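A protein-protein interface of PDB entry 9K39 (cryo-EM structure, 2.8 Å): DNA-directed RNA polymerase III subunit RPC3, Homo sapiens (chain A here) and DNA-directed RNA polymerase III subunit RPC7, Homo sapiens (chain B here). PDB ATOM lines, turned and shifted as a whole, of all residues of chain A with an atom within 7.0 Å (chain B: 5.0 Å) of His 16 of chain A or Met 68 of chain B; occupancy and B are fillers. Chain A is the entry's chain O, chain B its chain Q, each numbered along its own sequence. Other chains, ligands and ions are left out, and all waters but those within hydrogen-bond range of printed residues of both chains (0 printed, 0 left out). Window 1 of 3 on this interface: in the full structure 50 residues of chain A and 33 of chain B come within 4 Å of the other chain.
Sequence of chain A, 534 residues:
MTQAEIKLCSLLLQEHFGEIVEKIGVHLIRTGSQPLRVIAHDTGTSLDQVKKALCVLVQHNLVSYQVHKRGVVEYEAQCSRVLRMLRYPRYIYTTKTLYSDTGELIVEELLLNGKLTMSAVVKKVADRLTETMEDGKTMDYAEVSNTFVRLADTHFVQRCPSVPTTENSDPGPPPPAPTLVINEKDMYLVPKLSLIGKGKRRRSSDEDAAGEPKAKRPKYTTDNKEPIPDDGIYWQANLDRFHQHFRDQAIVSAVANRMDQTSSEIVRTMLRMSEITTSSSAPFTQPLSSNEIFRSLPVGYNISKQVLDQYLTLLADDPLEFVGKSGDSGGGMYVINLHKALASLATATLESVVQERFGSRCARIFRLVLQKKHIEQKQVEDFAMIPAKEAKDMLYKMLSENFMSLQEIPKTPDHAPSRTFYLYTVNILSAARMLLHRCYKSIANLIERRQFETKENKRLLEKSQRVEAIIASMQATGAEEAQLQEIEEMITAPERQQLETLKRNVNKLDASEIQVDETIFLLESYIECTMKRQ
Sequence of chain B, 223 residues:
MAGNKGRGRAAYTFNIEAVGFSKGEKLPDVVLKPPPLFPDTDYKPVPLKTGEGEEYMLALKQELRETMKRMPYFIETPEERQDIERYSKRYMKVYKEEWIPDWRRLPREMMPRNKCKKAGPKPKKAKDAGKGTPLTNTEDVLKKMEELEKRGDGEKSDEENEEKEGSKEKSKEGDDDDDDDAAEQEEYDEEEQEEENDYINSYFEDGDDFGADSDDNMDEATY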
ATOM      1  N   SER A  10     -11.772 -13.468   8.282  1.00  0.00           N
ATOM      2  CA  SER A  10     -10.472 -12.854   8.031  1.00  0.00           C
ATOM      3  C   SER A  10     -10.365 -11.504   8.725  1.00  0.00           C
ATOM      4  O   SER A  10      -9.360 -11.208   9.381  1.00  0.00           O
ATOM      5  CB  SER A  10     -10.247 -12.705   6.527  1.00  0.00           C
ATOM      6  OG  SER A  10      -8.991 -12.106   6.255  1.00  0.00           O
ATOM      7  N   LEU A  11     -11.397 -10.669   8.584  1.00  0.00           N
ATOM      8  CA  LEU A  11     -11.383  -9.362   9.233  1.00  0.00           C
ATOM      9  C   LEU A  11     -11.306  -9.499  10.751  1.00  0.00           C
ATOM     10  O   LEU A  11     -10.548  -8.774  11.408  1.00  0.00           O
ATOM     11  CB  LEU A  11     -12.619  -8.558   8.827  1.00  0.00           C
ATOM     12  CG  LEU A  11     -12.714  -8.160   7.353  1.00  0.00           C
ATOM     13  CD1 LEU A  11     -13.993  -7.383   7.091  1.00  0.00           C
ATOM     14  CD2 LEU A  11     -11.495  -7.352   6.935  1.00  0.00           C
ATOM     15  N   LEU A  12     -12.074 -10.430  11.320  1.00  0.00           N
ATOM     16  CA  LEU A  12     -12.063 -10.611  12.769  1.00  0.00           C
ATOM     17  C   LEU A  12     -10.703 -11.093  13.261  1.00  0.00           C
ATOM     18  O   LEU A  12     -10.180 -10.580  14.259  1.00  0.00           O
ATOM     19  CB  LEU A  12     -13.161 -11.589  13.186  1.00  0.00           C
ATOM     20  CG  LEU A  12     -14.602 -11.095  13.037  1.00  0.00           C
ATOM     21  CD1 LEU A  12     -15.586 -12.159  13.497  1.00  0.00           C
ATOM     22  CD2 LEU A  12     -14.805  -9.799  13.808  1.00  0.00           C
ATOM     23  N   LEU A  13     -10.111 -12.073  12.574  1.00  0.00           N
ATOM     24  CA  LEU A  13      -8.815 -12.591  12.998  1.00  0.00           C
ATOM     25  C   LEU A  13      -7.714 -11.554  12.815  1.00  0.00           C
ATOM     26  O   LEU A  13      -6.753 -11.523  13.588  1.00  0.00           O
ATOM     27  CB  LEU A  13      -8.485 -13.872  12.231  1.00  0.00           C
ATOM     28  CG  LEU A  13      -9.372 -15.084  12.528  1.00  0.00           C
ATOM     29  CD1 LEU A  13      -8.940 -16.282  11.698  1.00  0.00           C
ATOM     30  CD2 LEU A  13      -9.345 -15.419  14.012  1.00  0.00           C
ATOM     31  N   GLN A  14      -7.832 -10.698  11.796  1.00  0.00           N
ATOM     32  CA  GLN A  14      -6.841  -9.646  11.605  1.00  0.00           C
ATOM     33  C   GLN A  14      -6.968  -8.570  12.677  1.00  0.00           C
ATOM     34  O   GLN A  14      -5.958  -8.062  13.176  1.00  0.00           O
ATOM     35  CB  GLN A  14      -6.986  -9.035  10.211  1.00  0.00           C
ATOM     36  CG  GLN A  14      -5.949  -7.974   9.883  1.00  0.00           C
ATOM     37  CD  GLN A  14      -6.107  -7.424   8.480  1.00  0.00           C
ATOM     38  OE1 GLN A  14      -7.001  -7.832   7.739  1.00  0.00           O
ATOM     39  NE2 GLN A  14      -5.235  -6.495   8.106  1.00  0.00           N
ATOM     40  N   GLU A  15      -8.200  -8.213  13.046  1.00  0.00           N
ATOM     41  CA  GLU A  15      -8.396  -7.178  14.057  1.00  0.00           C
ATOM     42  C   GLU A  15      -8.103  -7.692  15.460  1.00  0.00           C
ATOM     43  O   GLU A  15      -7.777  -6.902  16.355  1.00  0.00           O
ATOM     44  CB  GLU A  15      -9.820  -6.630  13.972  1.00  0.00           C
ATOM     45  CG  GLU A  15     -10.090  -5.407  14.839  1.00  0.00           C
ATOM     46  CD  GLU A  15      -9.369  -4.165  14.347  1.00  0.00           C
ATOM     47  OE1 GLU A  15      -8.989  -4.124  13.158  1.00  0.00           O
ATOM     48  OE2 GLU A  15      -9.184  -3.228  15.153  1.00  0.00           O
ATOM     49  N   HIS A  16      -8.204  -9.004  15.678  1.00  0.00           N
ATOM     50  CA  HIS A  16      -8.106  -9.570  17.017  1.00  0.00           C
ATOM     51  C   HIS A  16      -6.798 -10.288  17.306  1.00  0.00           C
ATOM     52  O   HIS A  16      -6.359 -10.292  18.458  1.00  0.00           O
ATOM     53  CB  HIS A  16      -9.262 -10.548  17.264  1.00  0.00           C
ATOM     54  CG  HIS A  16     -10.611  -9.897  17.291  1.00  0.00           C
ATOM     55  ND1 HIS A  16     -11.779 -10.608  17.462  1.00  0.00           N
ATOM     56  CD2 HIS A  16     -10.977  -8.597  17.174  1.00  0.00           C
ATOM     57  CE1 HIS A  16     -12.806  -9.779  17.447  1.00  0.00           C
ATOM     58  NE2 HIS A  16     -12.345  -8.551  17.273  1.00  0.00           N
ATOM     59  N   PHE A  17      -6.158 -10.896  16.305  1.00  0.00           N
ATOM     60  CA  PHE A  17      -5.011 -11.753  16.584  1.00  0.00           C
ATOM     61  C   PHE A  17      -3.752 -11.320  15.841  1.00  0.00           C
ATOM     62  O   PHE A  17      -2.644 -11.459  16.368  1.00  0.00           O
ATOM     63  CB  PHE A  17      -5.350 -13.207  16.248  1.00  0.00           C
ATOM     64  CG  PHE A  17      -6.267 -13.860  17.244  1.00  0.00           C
ATOM     65  CD1 PHE A  17      -6.275 -13.453  18.569  1.00  0.00           C
ATOM     66  CD2 PHE A  17      -7.117 -14.881  16.859  1.00  0.00           C
ATOM     67  CE1 PHE A  17      -7.115 -14.052  19.488  1.00  0.00           C
ATOM     68  CE2 PHE A  17      -7.959 -15.484  17.773  1.00  0.00           C
ATOM     69  CZ  PHE A  17      -7.958 -15.067  19.089  1.00  0.00           C
ATOM     70  N   GLY A  18      -3.903 -10.796  14.624  1.00  0.00           N
ATOM     71  CA  GLY A  18      -2.763 -10.328  13.871  1.00  0.00           C
ATOM     72  C   GLY A  18      -2.848 -10.754  12.423  1.00  0.00           C
ATOM     73  O   GLY A  18      -3.926 -11.080  11.912  1.00  0.00           O
ATOM     74  N   VAL A  21      -1.282 -14.985  11.728  1.00  0.00           N
ATOM     75  CA  VAL A  21      -2.205 -15.992  12.238  1.00  0.00           C
ATOM     76  C   VAL A  21      -3.519 -15.987  11.464  1.00  0.00           C
ATOM     77  O   VAL A  21      -4.128 -17.039  11.250  1.00  0.00           O
ATOM     78  CB  VAL A  21      -2.427 -15.772  13.749  1.00  0.00           C
ATOM     79  CG1 VAL A  21      -2.759 -14.316  14.030  1.00  0.00           C
ATOM     80  CG2 VAL A  21      -3.520 -16.691  14.279  1.00  0.00           C
ATOM     81  N   HIS A  60      -7.730 -20.592  21.859  1.00  0.00           N
ATOM     82  CA  HIS A  60      -9.049 -19.978  21.910  1.00  0.00           C
ATOM     83  C   HIS A  60     -10.146 -20.893  21.377  1.00  0.00           C
ATOM     84  O   HIS A  60     -11.251 -20.417  21.099  1.00  0.00           O
ATOM     85  CB  HIS A  60      -9.050 -18.659  21.132  1.00  0.00           C
ATOM     86  CG  HIS A  60      -8.175 -17.603  21.727  1.00  0.00           C
ATOM     87  ND1 HIS A  60      -6.802 -17.722  21.793  1.00  0.00           N
ATOM     88  CD2 HIS A  60      -8.474 -16.407  22.289  1.00  0.00           C
ATOM     89  CE1 HIS A  60      -6.295 -16.645  22.365  1.00  0.00           C
ATOM     90  NE2 HIS A  60      -7.288 -15.832  22.676  1.00  0.00           N
ATOM     91  N   VAL A  82     -15.449 -18.834  15.007  1.00  0.00           N
ATOM     92  CA  VAL A  82     -14.918 -17.527  14.629  1.00  0.00           C
ATOM     93  C   VAL A  82     -16.055 -16.526  14.447  1.00  0.00           C
ATOM     94  O   VAL A  82     -15.901 -15.331  14.729  1.00  0.00           O
ATOM     95  CB  VAL A  82     -14.055 -17.644  13.359  1.00  0.00           C
ATOM     96  CG1 VAL A  82     -13.342 -16.328  13.083  1.00  0.00           C
ATOM     97  CG2 VAL A  82     -13.050 -18.777  13.504  1.00  0.00           C
ATOM     98  N   MET A  85     -17.257 -15.511  17.868  1.00  0.00           N
ATOM     99  CA  MET A  85     -16.308 -14.602  18.509  1.00  0.00           C
ATOM    100  C   MET A  85     -16.817 -13.163  18.513  1.00  0.00           C
ATOM    101  O   MET A  85     -16.534 -12.407  19.450  1.00  0.00           O
ATOM    102  CB  MET A  85     -14.954 -14.687  17.801  1.00  0.00           C
ATOM    103  CG  MET A  85     -13.937 -13.648  18.259  1.00  0.00           C
ATOM    104  SD  MET A  85     -12.362 -13.768  17.388  1.00  0.00           S
ATOM    105  CE  MET A  85     -11.798 -15.375  17.936  1.00  0.00           C
ATOM    106  N   LEU A  86     -17.578 -12.772  17.488  1.00  0.00           N
ATOM    107  CA  LEU A  86     -18.122 -11.420  17.430  1.00  0.00           C
ATOM    108  C   LEU A  86     -19.143 -11.154  18.530  1.00  0.00           C
ATOM    109  O   LEU A  86     -19.360  -9.991  18.891  1.00  0.00           O
ATOM    110  CB  LEU A  86     -18.753 -11.177  16.057  1.00  0.00           C
ATOM    111  CG  LEU A  86     -19.298  -9.777  15.756  1.00  0.00           C
ATOM    112  CD1 LEU A  86     -18.205  -8.735  15.933  1.00  0.00           C
ATOM    113  CD2 LEU A  86     -19.884  -9.715  14.357  1.00  0.00           C
ATOM    114  N   TYR A  88     -18.899 -11.635  21.627  1.00  0.00           N
ATOM    115  CA  TYR A  88     -18.296 -11.462  22.949  1.00  0.00           C
ATOM    116  C   TYR A  88     -18.890 -10.295  23.730  1.00  0.00           C
ATOM    117  O   TYR A  88     -19.195 -10.478  24.923  1.00  0.00           O
ATOM    118  CB  TYR A  88     -16.773 -11.323  22.813  1.00  0.00           C
ATOM    119  CG  TYR A  88     -16.058 -12.604  22.446  1.00  0.00           C
ATOM    120  CD1 TYR A  88     -16.728 -13.821  22.426  1.00  0.00           C
ATOM    121  CD2 TYR A  88     -14.707 -12.594  22.125  1.00  0.00           C
ATOM    122  CE1 TYR A  88     -16.070 -14.992  22.093  1.00  0.00           C
ATOM    123  CE2 TYR A  88     -14.044 -13.759  21.791  1.00  0.00           C
ATOM    124  CZ  TYR A  88     -14.729 -14.954  21.776  1.00  0.00           C
ATOM    125  OH  TYR A  88     -14.073 -16.117  21.445  1.00  0.00           O
ATOM    126  N   LEU A 111     -13.143 -15.431  27.822  1.00  0.00           N
ATOM    127  CA  LEU A 111     -13.235 -15.185  26.387  1.00  0.00           C
ATOM    128  C   LEU A 111     -11.925 -14.642  25.830  1.00  0.00           C
ATOM    129  O   LEU A 111     -11.568 -14.930  24.680  1.00  0.00           O
ATOM    130  CB  LEU A 111     -14.389 -14.225  26.091  1.00  0.00           C
ATOM    131  CG  LEU A 111     -15.793 -14.786  26.324  1.00  0.00           C
ATOM    132  CD1 LEU A 111     -16.852 -13.745  25.996  1.00  0.00           C
ATOM    133  CD2 LEU A 111     -16.005 -16.048  25.503  1.00  0.00           C
ATOM    134  N   LEU A 112     -11.196 -13.853  26.621  1.00  0.00           N
ATOM    135  CA  LEU A 112      -9.936 -13.289  26.146  1.00  0.00           C
ATOM    136  C   LEU A 112      -8.790 -14.291  26.189  1.00  0.00           C
ATOM    137  O   LEU A 112      -7.796 -14.108  25.478  1.00  0.00           O
ATOM    138  CB  LEU A 112      -9.572 -12.046  26.959  1.00  0.00           C
ATOM    139  CG  LEU A 112     -10.011 -10.693  26.394  1.00  0.00           C
ATOM    140  CD1 LEU A 112     -11.519 -10.641  26.186  1.00  0.00           C
ATOM    141  CD2 LEU A 112      -9.551  -9.561  27.297  1.00  0.00           C
ATOM    142  N   ARG A 450     -14.701   0.909   8.940  1.00  0.00           N
ATOM    143  CA  ARG A 450     -14.072   1.360  10.177  1.00  0.00           C
ATOM    144  C   ARG A 450     -12.553   1.304  10.074  1.00  0.00           C
ATOM    145  O   ARG A 450     -11.860   2.248  10.476  1.00  0.00           O
ATOM    146  CB  ARG A 450     -14.555   0.521  11.361  1.00  0.00           C
ATOM    147  CG  ARG A 450     -14.108   1.064  12.710  1.00  0.00           C
ATOM    148  CD  ARG A 450     -14.226   0.026  13.814  1.00  0.00           C
ATOM    149  NE  ARG A 450     -13.201  -1.011  13.708  1.00  0.00           N
ATOM    150  CZ  ARG A 450     -13.403  -2.212  13.181  1.00  0.00           C
ATOM    151  NH1 ARG A 450     -14.597  -2.543  12.711  1.00  0.00           N
ATOM    152  NH2 ARG A 450     -12.408  -3.089  13.129  1.00  0.00           N
ATOM    153  N   GLU A 513     -22.639  -2.640  13.955  1.00  0.00           N
ATOM    154  CA  GLU A 513     -22.070  -3.980  13.861  1.00  0.00           C
ATOM    155  C   GLU A 513     -22.563  -4.867  14.998  1.00  0.00           C
ATOM    156  O   GLU A 513     -22.802  -6.066  14.804  1.00  0.00           O
ATOM    157  CB  GLU A 513     -20.543  -3.896  13.866  1.00  0.00           C
ATOM    158  CG  GLU A 513     -19.832  -5.238  13.859  1.00  0.00           C
ATOM    159  CD  GLU A 513     -18.324  -5.093  13.902  1.00  0.00           C
ATOM    160  OE1 GLU A 513     -17.831  -3.954  13.763  1.00  0.00           O
ATOM    161  OE2 GLU A 513     -17.630  -6.116  14.081  1.00  0.00           O
ATOM    162  N   GLU B  63     -13.032  -1.386  24.274  1.00  0.00           N
ATOM    163  CA  GLU B  63     -12.038  -1.819  25.251  1.00  0.00           C
ATOM    164  C   GLU B  63     -11.402  -3.142  24.844  1.00  0.00           C
ATOM    165  O   GLU B  63     -10.194  -3.334  25.016  1.00  0.00           O
ATOM    166  CB  GLU B  63     -12.677  -1.936  26.636  1.00  0.00           C
ATOM    167  CG  GLU B  63     -13.054  -0.605  27.266  1.00  0.00           C
ATOM    168  CD  GLU B  63     -13.728  -0.766  28.614  1.00  0.00           C
ATOM    169  OE1 GLU B  63     -13.916  -1.919  29.054  1.00  0.00           O
ATOM    170  OE2 GLU B  63     -14.070   0.262  29.235  1.00  0.00           O
ATOM    171  N   LEU B  64     -12.201  -4.065  24.307  1.00  0.00           N
ATOM    172  CA  LEU B  64     -11.653  -5.337  23.844  1.00  0.00           C
ATOM    173  C   LEU B  64     -10.711  -5.128  22.664  1.00  0.00           C
ATOM    174  O   LEU B  64      -9.643  -5.747  22.599  1.00  0.00           O
ATOM    175  CB  LEU B  64     -12.783  -6.296  23.464  1.00  0.00           C
ATOM    176  CG  LEU B  64     -13.661  -6.800  24.612  1.00  0.00           C
ATOM    177  CD1 LEU B  64     -14.645  -7.846  24.114  1.00  0.00           C
ATOM    178  CD2 LEU B  64     -12.805  -7.355  25.742  1.00  0.00           C
ATOM    179  N   ARG B  65     -11.092  -4.264  21.718  1.00  0.00           N
ATOM    180  CA  ARG B  65     -10.199  -3.930  20.613  1.00  0.00           C
ATOM    181  C   ARG B  65      -8.878  -3.371  21.129  1.00  0.00           C
ATOM    182  O   ARG B  65      -7.805  -3.701  20.614  1.00  0.00           O
ATOM    183  CB  ARG B  65     -10.866  -2.928  19.672  1.00  0.00           C
ATOM    184  CG  ARG B  65     -11.864  -3.523  18.696  1.00  0.00           C
ATOM    185  CD  ARG B  65     -12.055  -2.588  17.511  1.00  0.00           C
ATOM    186  NE  ARG B  65     -13.099  -3.038  16.597  1.00  0.00           N
ATOM    187  CZ  ARG B  65     -14.345  -2.571  16.602  1.00  0.00           C
ATOM    188  NH1 ARG B  65     -14.700  -1.640  17.474  1.00  0.00           N
ATOM    189  NH2 ARG B  65     -15.230  -3.038  15.733  1.00  0.00           N
ATOM    190  N   GLU B  66      -8.942  -2.510  22.150  1.00  0.00           N
ATOM    191  CA  GLU B  66      -7.723  -1.887  22.657  1.00  0.00           C
ATOM    192  C   GLU B  66      -6.872  -2.859  23.469  1.00  0.00           C
ATOM    193  O   GLU B  66      -5.642  -2.736  23.479  1.00  0.00           O
ATOM    194  CB  GLU B  66      -8.072  -0.662  23.503  1.00  0.00           C
ATOM    195  CG  GLU B  66      -8.706   0.476  22.718  1.00  0.00           C
ATOM    196  CD  GLU B  66      -9.000   1.686  23.583  1.00  0.00           C
ATOM    197  OE1 GLU B  66      -8.729   1.627  24.800  1.00  0.00           O
ATOM    198  OE2 GLU B  66      -9.500   2.695  23.045  1.00  0.00           O
ATOM    199  N   THR B  67      -7.494  -3.823  24.147  1.00  0.00           N
ATOM    200  CA  THR B  67      -6.755  -4.689  25.060  1.00  0.00           C
ATOM    201  C   THR B  67      -6.319  -6.006  24.432  1.00  0.00           C
ATOM    202  O   THR B  67      -5.429  -6.669  24.976  1.00  0.00           O
ATOM    203  CB  THR B  67      -7.593  -4.980  26.311  1.00  0.00           C
ATOM    204  OG1 THR B  67      -6.748  -5.514  27.337  1.00  0.00           O
ATOM    205  CG2 THR B  67      -8.692  -5.987  26.003  1.00  0.00           C
ATOM    206  N   MET B  68      -6.913  -6.409  23.309  1.00  0.00           N
ATOM    207  CA  MET B  68      -6.566  -7.682  22.692  1.00  0.00           C
ATOM    208  C   MET B  68      -5.385  -7.583  21.738  1.00  0.00           C
ATOM    209  O   MET B  68      -4.789  -8.612  21.405  1.00  0.00           O
ATOM    210  CB  MET B  68      -7.787  -8.253  21.959  1.00  0.00           C
ATOM    211  CG  MET B  68      -7.684  -9.730  21.611  1.00  0.00           C
ATOM    212  SD  MET B  68      -9.297 -10.501  21.380  1.00  0.00           S
ATOM    213  CE  MET B  68     -10.050  -9.364  20.218  1.00  0.00           C
ATOM    214  N   LYS B  69      -5.022  -6.376  21.299  1.00  0.00           N
ATOM    215  CA  LYS B  69      -3.846  -6.227  20.448  1.00  0.00           C
ATOM    216  C   LYS B  69      -2.558  -6.330  21.256  1.00  0.00           C
ATOM    217  O   LYS B  69      -1.554  -6.856  20.766  1.00  0.00           O
ATOM    218  CB  LYS B  69      -3.902  -4.897  19.695  1.00  0.00           C
ATOM    219  CG  LYS B  69      -5.094  -4.762  18.764  1.00  0.00           C
ATOM    220  CD  LYS B  69      -4.973  -3.526  17.887  1.00  0.00           C
ATOM    221  CE  LYS B  69      -4.839  -2.265  18.723  1.00  0.00           C
ATOM    222  NZ  LYS B  69      -4.695  -1.048  17.877  1.00  0.00           N
ATOM    223  N   ARG B  70      -2.572  -5.834  22.495  1.00  0.00           N
ATOM    224  CA  ARG B  70      -1.427  -5.968  23.385  1.00  0.00           C
ATOM    225  C   ARG B  70      -1.368  -7.328  24.069  1.00  0.00           C
ATOM    226  O   ARG B  70      -0.388  -7.612  24.765  1.00  0.00           O
ATOM    227  CB  ARG B  70      -1.453  -4.859  24.442  1.00  0.00           C
ATOM    228  CG  ARG B  70      -1.213  -3.465  23.879  1.00  0.00           C
ATOM    229  CD  ARG B  70      -1.386  -2.385  24.938  1.00  0.00           C
ATOM    230  NE  ARG B  70      -2.789  -2.150  25.269  1.00  0.00           N
ATOM    231  CZ  ARG B  70      -3.409  -2.671  26.326  1.00  0.00           C
ATOM    232  NH1 ARG B  70      -2.751  -3.456  27.164  1.00  0.00           N
ATOM    233  NH2 ARG B  70      -4.688  -2.399  26.545  1.00  0.00           N
ATOM    234  N   MET B  71      -2.386  -8.164  23.890  1.00  0.00           N
ATOM    235  CA  MET B  71      -2.366  -9.497  24.471  1.00  0.00           C
ATOM    236  C   MET B  71      -1.301 -10.345  23.774  1.00  0.00           C
ATOM    237  O   MET B  71      -1.109 -10.223  22.558  1.00  0.00           O
ATOM    238  CB  MET B  71      -3.742 -10.155  24.333  1.00  0.00           C
ATOM    239  CG  MET B  71      -3.949 -11.380  25.207  1.00  0.00           C
ATOM    240  SD  MET B  71      -3.943 -10.986  26.966  1.00  0.00           S
ATOM    241  CE  MET B  71      -4.137 -12.616  27.678  1.00  0.00           C
ATOM    242  N   PHE B  74      -2.081 -12.005  20.436  1.00  0.00           N
ATOM    243  CA  PHE B  74      -1.971 -11.208  19.216  1.00  0.00           C
ATOM    244  C   PHE B  74      -0.516 -11.212  18.767  1.00  0.00           C
ATOM    245  O   PHE B  74       0.287 -10.387  19.213  1.00  0.00           O
ATOM    246  CB  PHE B  74      -2.473  -9.790  19.459  1.00  0.00           C
ATOM    247  CG  PHE B  74      -2.503  -8.933  18.226  1.00  0.00           C
ATOM    248  CD1 PHE B  74      -3.622  -8.910  17.408  1.00  0.00           C
ATOM    249  CD2 PHE B  74      -1.418  -8.137  17.888  1.00  0.00           C
ATOM    250  CE1 PHE B  74      -3.654  -8.121  16.275  1.00  0.00           C
ATOM    251  CE2 PHE B  74      -1.445  -7.346  16.755  1.00  0.00           C
ATOM    252  CZ  PHE B  74      -2.565  -7.337  15.947  1.00  0.00           C
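The side-chain carboxylate of Glu 513 of chain A lies within salt-bridge range of the guanidinium group of Arg 65 of chain B (3.4 Å). The guanidinium group (NH1) of Arg 450 of chain A sits close to the guanidinium group (NH2) of Arg 65 of chain B (3.1 Å).
OE1 of Glu 513 of chain A lies within salt-bridge range of NH1 of Arg 450 of chain A, at 3.7 Å. ND1 of His 16 of chain A is in hydrogen-bond range of SD of Met 85 of chain A (3.2 Å). O of Leu 13 of chain A sits at hydrogen-bond distance from N of Gly 18 of chain A (3.1 Å). A ring nitrogen (NE2) of His 60 of chain A is in hydrogen-bond range of the backbone carbonyl oxygen (O) of Leu 112 of chain A. The side-chain carboxylate of Glu 15 of chain A is in salt-bridge range of the guanidinium group of Arg 450 of chain A, at 3.6 Å.
Among the printed residues, pairs that only touch across the chains: Phe 17 of chain A with Phe 74 of chain B, His 16 of chain A with Met 68 of chain B, Gly 18 of chain A with Phe 74 of chain B, His 16 of chain A with Phe 74 of chain B, Leu 112 of chain A with Leu 64 of chain B, Glu 15 of chain A with Arg 65 of chain B, Gln 14 of chain A with Phe 74 of chain B and Leu 112 of chain A with Thr 67 of chain B.
Printed residues of chain A within 4 Å of Phe 74 of chain B: Gln 14 (3.9 Å), His 16 (3.2 Å), Phe 17 (2.9 Å) and Gly 18 (3.2 Å). Of the printed residues of chain B, Gln 14 of chain A touches Phe 74 (3.9 Å). Lys 69 of chain B touches none of the printed residues of chain A. The nearest printed residue of chain B that does not touch His 16 of chain A is Lys 69 of chain B (5.0 Å).
Hydrophobic or aromatic side chains of chain B that line the printed part of chain A: Leu 64, Met 68 and Phe 74. Hydrophobic or aromatic side chains of chain A within 4 Å of the printed part of chain B: His 16 and Leu 112. Among the printed residues, 10 pairs touch across the chains. Among the printed residues, Asp or Glu carboxylates within 4 Å of a Lys or Arg side-chain nitrogen of the other chain: Glu 513 of chain A with Arg 65 of chain B (3.4 Å).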
